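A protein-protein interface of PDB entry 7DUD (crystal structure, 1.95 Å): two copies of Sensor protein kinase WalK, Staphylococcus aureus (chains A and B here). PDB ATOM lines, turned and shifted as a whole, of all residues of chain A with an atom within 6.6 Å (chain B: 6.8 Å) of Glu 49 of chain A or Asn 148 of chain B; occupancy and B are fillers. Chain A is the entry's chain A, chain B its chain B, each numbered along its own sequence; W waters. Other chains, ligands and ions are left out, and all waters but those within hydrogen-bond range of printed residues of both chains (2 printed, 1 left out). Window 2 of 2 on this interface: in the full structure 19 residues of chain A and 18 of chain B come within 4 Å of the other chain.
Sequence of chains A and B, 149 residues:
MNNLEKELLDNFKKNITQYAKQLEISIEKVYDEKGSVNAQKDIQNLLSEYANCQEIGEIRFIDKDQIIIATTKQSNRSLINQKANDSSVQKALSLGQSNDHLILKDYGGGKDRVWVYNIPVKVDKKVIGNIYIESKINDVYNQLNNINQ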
ATOM      1  N   TYR A  19       0.697  -5.612 -31.890  1.00  0.00           N
ATOM      2  CA  TYR A  19       1.544  -4.752 -31.061  1.00  0.00           C
ATOM      3  C   TYR A  19       0.721  -4.032 -29.983  1.00  0.00           C
ATOM      4  O   TYR A  19       1.085  -4.000 -28.793  1.00  0.00           O
ATOM      5  CB  TYR A  19       2.226  -3.764 -32.013  1.00  0.00           C
ATOM      6  CG  TYR A  19       3.352  -2.886 -31.505  1.00  0.00           C
ATOM      7  CD1 TYR A  19       4.594  -3.423 -31.201  1.00  0.00           C
ATOM      8  CD2 TYR A  19       3.172  -1.506 -31.365  1.00  0.00           C
ATOM      9  CE1 TYR A  19       5.621  -2.638 -30.760  1.00  0.00           C
ATOM     10  CE2 TYR A  19       4.200  -0.700 -30.893  1.00  0.00           C
ATOM     11  CZ  TYR A  19       5.431  -1.278 -30.610  1.00  0.00           C
ATOM     12  OH  TYR A  19       6.492  -0.504 -30.166  1.00  0.00           O
ATOM     13  N   GLN A  44       2.838   6.068 -18.849  1.00  0.00           N
ATOM     14  CA  GLN A  44       3.615   6.922 -19.739  1.00  0.00           C
ATOM     15  C   GLN A  44       4.833   6.192 -20.290  1.00  0.00           C
ATOM     16  O   GLN A  44       5.102   6.239 -21.495  1.00  0.00           O
ATOM     17  CB  GLN A  44       4.031   8.195 -19.010  1.00  0.00           C
ATOM     18  CG  GLN A  44       4.744   9.175 -19.899  1.00  0.00           C
ATOM     19  CD  GLN A  44       3.867   9.695 -21.008  1.00  0.00           C
ATOM     20  OE1 GLN A  44       2.981  10.512 -20.780  1.00  0.00           O
ATOM     21  NE2 GLN A  44       4.146   9.267 -22.233  1.00  0.00           N
ATOM     22  N   ASN A  45       5.590   5.510 -19.425  1.00  0.00           N
ATOM     23  CA  ASN A  45       6.794   4.840 -19.905  1.00  0.00           C
ATOM     24  C   ASN A  45       6.456   3.744 -20.903  1.00  0.00           C
ATOM     25  O   ASN A  45       7.156   3.573 -21.906  1.00  0.00           O
ATOM     26  CB  ASN A  45       7.603   4.285 -18.733  1.00  0.00           C
ATOM     27  CG  ASN A  45       7.956   5.356 -17.722  1.00  0.00           C
ATOM     28  OD1 ASN A  45       8.028   5.100 -16.522  1.00  0.00           O
ATOM     29  ND2 ASN A  45       8.153   6.578 -18.207  1.00  0.00           N
ATOM     30  N   LEU A  46       5.363   3.013 -20.666  1.00  0.00           N
ATOM     31  CA  LEU A  46       4.962   1.968 -21.602  1.00  0.00           C
ATOM     32  C   LEU A  46       4.534   2.570 -22.935  1.00  0.00           C
ATOM     33  O   LEU A  46       4.883   2.052 -24.008  1.00  0.00           O
ATOM     34  CB  LEU A  46       3.831   1.137 -20.992  1.00  0.00           C
ATOM     35  CG  LEU A  46       4.248   0.021 -20.029  1.00  0.00           C
ATOM     36  CD1 LEU A  46       3.021  -0.549 -19.342  1.00  0.00           C
ATOM     37  CD2 LEU A  46       5.040  -1.084 -20.747  1.00  0.00           C
ATOM     38  N   LEU A  47       3.755   3.652 -22.888  1.00  0.00           N
ATOM     39  CA  LEU A  47       3.378   4.319 -24.124  1.00  0.00           C
ATOM     40  C   LEU A  47       4.619   4.759 -24.885  1.00  0.00           C
ATOM     41  O   LEU A  47       4.714   4.562 -26.096  1.00  0.00           O
ATOM     42  CB  LEU A  47       2.471   5.525 -23.846  1.00  0.00           C
ATOM     43  CG  LEU A  47       1.125   5.279 -23.154  1.00  0.00           C
ATOM     44  CD1 LEU A  47       0.233   6.502 -23.284  1.00  0.00           C
ATOM     45  CD2 LEU A  47       0.440   4.034 -23.652  1.00  0.00           C
ATOM     46  N   SER A  48       5.585   5.352 -24.179  1.00  0.00           N
ATOM     47  CA  SER A  48       6.784   5.867 -24.831  1.00  0.00           C
ATOM     48  C   SER A  48       7.607   4.755 -25.457  1.00  0.00           C
ATOM     49  O   SER A  48       8.146   4.924 -26.555  1.00  0.00           O
ATOM     50  CB  SER A  48       7.633   6.637 -23.828  1.00  0.00           C
ATOM     51  OG  SER A  48       6.925   7.765 -23.366  1.00  0.00           O
ATOM     52  N   GLU A  49       7.747   3.621 -24.757  1.00  0.00           N
ATOM     53  CA  GLU A  49       8.384   2.451 -25.350  1.00  0.00           C
ATOM     54  C   GLU A  49       7.717   2.086 -26.660  1.00  0.00           C
ATOM     55  O   GLU A  49       8.368   2.005 -27.712  1.00  0.00           O
ATOM     56  CB  GLU A  49       8.290   1.227 -24.432  1.00  0.00           C
ATOM     57  CG  GLU A  49       8.930   1.265 -23.095  1.00  0.00           C
ATOM     58  CD  GLU A  49       9.134  -0.154 -22.574  1.00  0.00           C
ATOM     59  OE1 GLU A  49       8.275  -1.033 -22.857  1.00  0.00           O
ATOM     60  OE2 GLU A  49      10.171  -0.409 -21.923  1.00  0.00           O
ATOM     61  N   TYR A  50       6.407   1.818 -26.594  1.00  0.00           N
ATOM     62  CA  TYR A  50       5.702   1.301 -27.763  1.00  0.00           C
ATOM     63  C   TYR A  50       5.664   2.300 -28.915  1.00  0.00           C
ATOM     64  O   TYR A  50       5.637   1.889 -30.080  1.00  0.00           O
ATOM     65  CB  TYR A  50       4.290   0.876 -27.368  1.00  0.00           C
ATOM     66  CG  TYR A  50       4.247  -0.512 -26.795  1.00  0.00           C
ATOM     67  CD1 TYR A  50       4.637  -0.759 -25.478  1.00  0.00           C
ATOM     68  CD2 TYR A  50       3.820  -1.581 -27.568  1.00  0.00           C
ATOM     69  CE1 TYR A  50       4.603  -2.060 -24.944  1.00  0.00           C
ATOM     70  CE2 TYR A  50       3.789  -2.882 -27.051  1.00  0.00           C
ATOM     71  CZ  TYR A  50       4.178  -3.103 -25.744  1.00  0.00           C
ATOM     72  OH  TYR A  50       4.147  -4.375 -25.262  1.00  0.00           O
ATOM     73  N   ALA A  51       5.658   3.598 -28.625  1.00  0.00           N
ATOM     74  CA  ALA A  51       5.603   4.624 -29.680  1.00  0.00           C
ATOM     75  C   ALA A  51       6.886   4.790 -30.368  1.00  0.00           C
ATOM     76  O   ALA A  51       7.061   5.672 -31.229  1.00  0.00           O
ATOM     77  CB  ALA A  51       5.178   5.973 -29.104  1.00  0.00           C
ATOM     78  N   ASN A  52       7.859   3.950 -30.067  1.00  0.00           N
ATOM     79  CA  ASN A  52       9.143   4.072 -30.728  1.00  0.00           C
ATOM     80  C   ASN A  52       9.163   3.181 -31.987  1.00  0.00           C
ATOM     81  O   ASN A  52      10.138   3.189 -32.747  1.00  0.00           O
ATOM     82  CB  ASN A  52      10.216   3.751 -29.668  1.00  0.00           C
ATOM     83  CG  ASN A  52      11.624   4.139 -30.071  1.00  0.00           C
ATOM     84  OD1 ASN A  52      11.874   4.648 -31.160  1.00  0.00           O
ATOM     85  ND2 ASN A  52      12.542   3.992 -29.127  1.00  0.00           N
ATOM     86  N   CYS A  53       8.078   2.423 -32.217  1.00  0.00           N
ATOM     87  CA  CYS A  53       7.806   1.734 -33.480  1.00  0.00           C
ATOM     88  C   CYS A  53       7.658   2.732 -34.618  1.00  0.00           C
ATOM     89  O   CYS A  53       7.028   3.782 -34.448  1.00  0.00           O
ATOM     90  CB  CYS A  53       6.509   0.920 -33.354  1.00  0.00           C
ATOM     91  SG  CYS A  53       5.730   0.340 -34.914  1.00  0.00           S
ATOM     92  N   ILE A  59       0.505   7.650 -29.786  1.00  0.00           N
ATOM     93  CA  ILE A  59      -0.305   6.838 -28.886  1.00  0.00           C
ATOM     94  C   ILE A  59      -0.788   7.729 -27.755  1.00  0.00           C
ATOM     95  O   ILE A  59      -0.043   8.582 -27.258  1.00  0.00           O
ATOM     96  CB  ILE A  59       0.443   5.609 -28.306  1.00  0.00           C
ATOM     97  CG1 ILE A  59       1.199   4.819 -29.376  1.00  0.00           C
ATOM     98  CG2 ILE A  59      -0.520   4.690 -27.547  1.00  0.00           C
ATOM     99  CD1 ILE A  59       2.062   3.674 -28.749  1.00  0.00           C
ATOM    100  N   THR A  72       2.337  10.361 -26.354  1.00  0.00           N
ATOM    101  CA  THR A  72       3.726  10.067 -26.677  1.00  0.00           C
ATOM    102  C   THR A  72       4.377  11.162 -27.527  1.00  0.00           C
ATOM    103  O   THR A  72       5.621  11.231 -27.588  1.00  0.00           O
ATOM    104  CB  THR A  72       3.805   8.710 -27.390  1.00  0.00           C
ATOM    105  OG1 THR A  72       3.173   8.788 -28.686  1.00  0.00           O
ATOM    106  CG2 THR A  72       3.106   7.651 -26.578  1.00  0.00           C
ATOM    107  N   GLN B 143      12.534  -3.897 -32.750  1.00  0.00           N
ATOM    108  CA  GLN B 143      11.263  -3.420 -32.226  1.00  0.00           C
ATOM    109  C   GLN B 143      10.848  -4.256 -31.021  1.00  0.00           C
ATOM    110  O   GLN B 143      10.491  -3.712 -29.968  1.00  0.00           O
ATOM    111  CB  GLN B 143      10.243  -3.474 -33.351  1.00  0.00           C
ATOM    112  CG  GLN B 143      10.560  -2.500 -34.486  1.00  0.00           C
ATOM    113  CD  GLN B 143       9.717  -2.795 -35.706  1.00  0.00           C
ATOM    114  OE1 GLN B 143       8.763  -3.568 -35.636  1.00  0.00           O
ATOM    115  NE2 GLN B 143      10.066  -2.199 -36.829  1.00  0.00           N
ATOM    116  N   LEU B 144      10.991  -5.581 -31.129  1.00  0.00           N
ATOM    117  CA  LEU B 144      10.664  -6.454 -30.009  1.00  0.00           C
ATOM    118  C   LEU B 144      11.522  -6.108 -28.808  1.00  0.00           C
ATOM    119  O   LEU B 144      11.014  -5.929 -27.689  1.00  0.00           O
ATOM    120  CB  LEU B 144      10.870  -7.918 -30.410  1.00  0.00           C
ATOM    121  CG  LEU B 144       9.768  -8.562 -31.256  1.00  0.00           C
ATOM    122  CD1 LEU B 144      10.323  -9.793 -31.962  1.00  0.00           C
ATOM    123  CD2 LEU B 144       8.488  -8.891 -30.451  1.00  0.00           C
ATOM    124  N   ASN B 145      12.832  -5.946 -29.029  1.00  0.00           N
ATOM    125  CA  ASN B 145      13.682  -5.688 -27.879  1.00  0.00           C
ATOM    126  C   ASN B 145      13.333  -4.360 -27.246  1.00  0.00           C
ATOM    127  O   ASN B 145      13.520  -4.189 -26.039  1.00  0.00           O
ATOM    128  CB  ASN B 145      15.166  -5.739 -28.256  1.00  0.00           C
ATOM    129  CG  ASN B 145      15.662  -7.161 -28.504  1.00  0.00           C
ATOM    130  OD1 ASN B 145      16.586  -7.378 -29.293  1.00  0.00           O
ATOM    131  ND2 ASN B 145      15.076  -8.134 -27.795  1.00  0.00           N
ATOM    132  N   ASN B 146      12.759  -3.437 -28.014  1.00  0.00           N
ATOM    133  CA  ASN B 146      12.461  -2.139 -27.424  1.00  0.00           C
ATOM    134  C   ASN B 146      11.233  -2.173 -26.516  1.00  0.00           C
ATOM    135  O   ASN B 146      11.094  -1.297 -25.649  1.00  0.00           O
ATOM    136  CB  ASN B 146      12.306  -1.101 -28.533  1.00  0.00           C
ATOM    137  CG  ASN B 146      11.968   0.278 -28.000  1.00  0.00           C
ATOM    138  OD1 ASN B 146      10.801   0.675 -27.980  1.00  0.00           O
ATOM    139  ND2 ASN B 146      12.981   1.006 -27.552  1.00  0.00           N
ATOM    140  N   ILE B 147      10.359  -3.167 -26.668  1.00  0.00           N
ATOM    141  CA  ILE B 147       9.210  -3.320 -25.788  1.00  0.00           C
ATOM    142  C   ILE B 147       9.409  -4.497 -24.829  1.00  0.00           C
ATOM    143  O   ILE B 147       8.472  -4.921 -24.142  1.00  0.00           O
ATOM    144  CB  ILE B 147       7.914  -3.414 -26.612  1.00  0.00           C
ATOM    145  CG1 ILE B 147       7.978  -4.564 -27.629  1.00  0.00           C
ATOM    146  CG2 ILE B 147       7.672  -2.088 -27.322  1.00  0.00           C
ATOM    147  CD1 ILE B 147       6.610  -5.064 -28.121  1.00  0.00           C
ATOM    148  N   ASN B 148      10.645  -4.986 -24.740  1.00  0.00           N
ATOM    149  CA  ASN B 148      11.020  -6.078 -23.847  1.00  0.00           C
ATOM    150  C   ASN B 148      10.157  -7.307 -24.119  1.00  0.00           C
ATOM    151  O   ASN B 148       9.506  -7.868 -23.234  1.00  0.00           O
ATOM    152  CB  ASN B 148      10.935  -5.640 -22.383  1.00  0.00           C
ATOM    153  CG  ASN B 148      11.804  -4.436 -22.088  1.00  0.00           C
ATOM    154  OD1 ASN B 148      13.025  -4.503 -22.190  1.00  0.00           O
ATOM    155  ND2 ASN B 148      11.179  -3.326 -21.726  1.00  0.00           N
ATOM    156  N   GLN B 149      10.156  -7.704 -25.386  1.00  0.00           N
ATOM    157  CA  GLN B 149       9.386  -8.840 -25.855  1.00  0.00           C
ATOM    158  C   GLN B 149      10.274  -9.747 -26.711  1.00  0.00           C
ATOM    159  O   GLN B 149       9.794 -10.719 -27.305  1.00  0.00           O
ATOM    160  CB  GLN B 149       8.147  -8.364 -26.648  1.00  0.00           C
ATOM    161  CG  GLN B 149       7.094  -7.654 -25.791  1.00  0.00           C
ATOM    162  CD  GLN B 149       6.426  -8.576 -24.770  1.00  0.00           C
ATOM    163  OE1 GLN B 149       6.432  -9.805 -24.928  1.00  0.00           O
ATOM    164  NE2 GLN B 149       5.864  -7.986 -23.706  1.00  0.00           N
HETATM  165  O   HOH W   1       9.117  -1.327 -30.587  1.00  0.00           O
HETATM  166  O   HOH W   2       5.964  -5.057 -23.379  1.00  0.00           O
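OD1 of Asn 146 of chain B lies close to O of Glu 49 of chain A. ND2 of Asn 148 of chain B is in hydrogen-bond range of OE2 of Glu 49 of chain A, 3.1 Å away. ND2 of Asn 146 of chain B sits close to ND2 of Asn 52 of chain A, 3.4 Å away.
The side-chain hydroxyl (OH) of Tyr 19 of chain A lies within hydrogen-bond range of the backbone carbonyl oxygen (O) of Tyr 50 of chain A, at 2.5 Å.
Among the printed residues, merely in contact across the chains: Tyr 19 of chain A with Ile 147 of chain B, Tyr 50 of chain A with Ile 147 of chain B and Glu 49 of chain A with Ile 147 of chain B.
Glu 49 of chain A touches just these residues of chain B: Asn 146, Ile 147 and Asn 148. Asn 148 of chain B touches one residue of chain A. Printed residues of chain A within 4 Å of Ile 147 of chain B: Tyr 19, Glu 49 and Tyr 50. Of the printed residues of chain B, Asn 52 of chain A touches Asn 146. Ile 59 of chain A touches none of the printed residues of chain B. Gln 44 of chain A touches none of the printed residues of chain B. The nearest printed residue of chain B that does not touch Glu 49 of chain A is Gln 143 of chain B (6.5 Å). The nearest residue of chain A that does not touch Asn 148 of chain B is Tyr 50 of chain A (6.5 Å). The nearest printed residue of chain B that does not touch Asn 52 of chain A is Gln 143 of chain B (6.0 Å).
Printed residues of chain B that touch a printed residue of chain A: Asn 146, Ile 147 and Asn 148. Hydrophobic or aromatic side chains of chain B that line the printed part of chain A: Ile 147. Of the 13 printed residues of chain A, 4 touch a printed residue of chain B. Hydrophobic or aromatic side chains of chain A within 4 Å of the printed part of chain B: Tyr 19 and Tyr 50. Among the printed residues, no Asp or Glu carboxylate lies within 4 Å of a Lys or Arg side-chain nitrogen of the other chain.
No position is printed for both chains.
Water W2 lies within hydrogen-bond range of the backbone carbonyl oxygen (O) of Ile 147 of chain B (2.6 Å), the side-chain hydroxyl (OH) of Tyr 50 of chain A (2.7 Å) and the side-chain amide nitrogen (NE2) of Gln 149 of chain B (2.9 Å). Water W1 lies within hydrogen-bond range of OH of Tyr 19 of chain A and O of Gln 143 of chain B.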
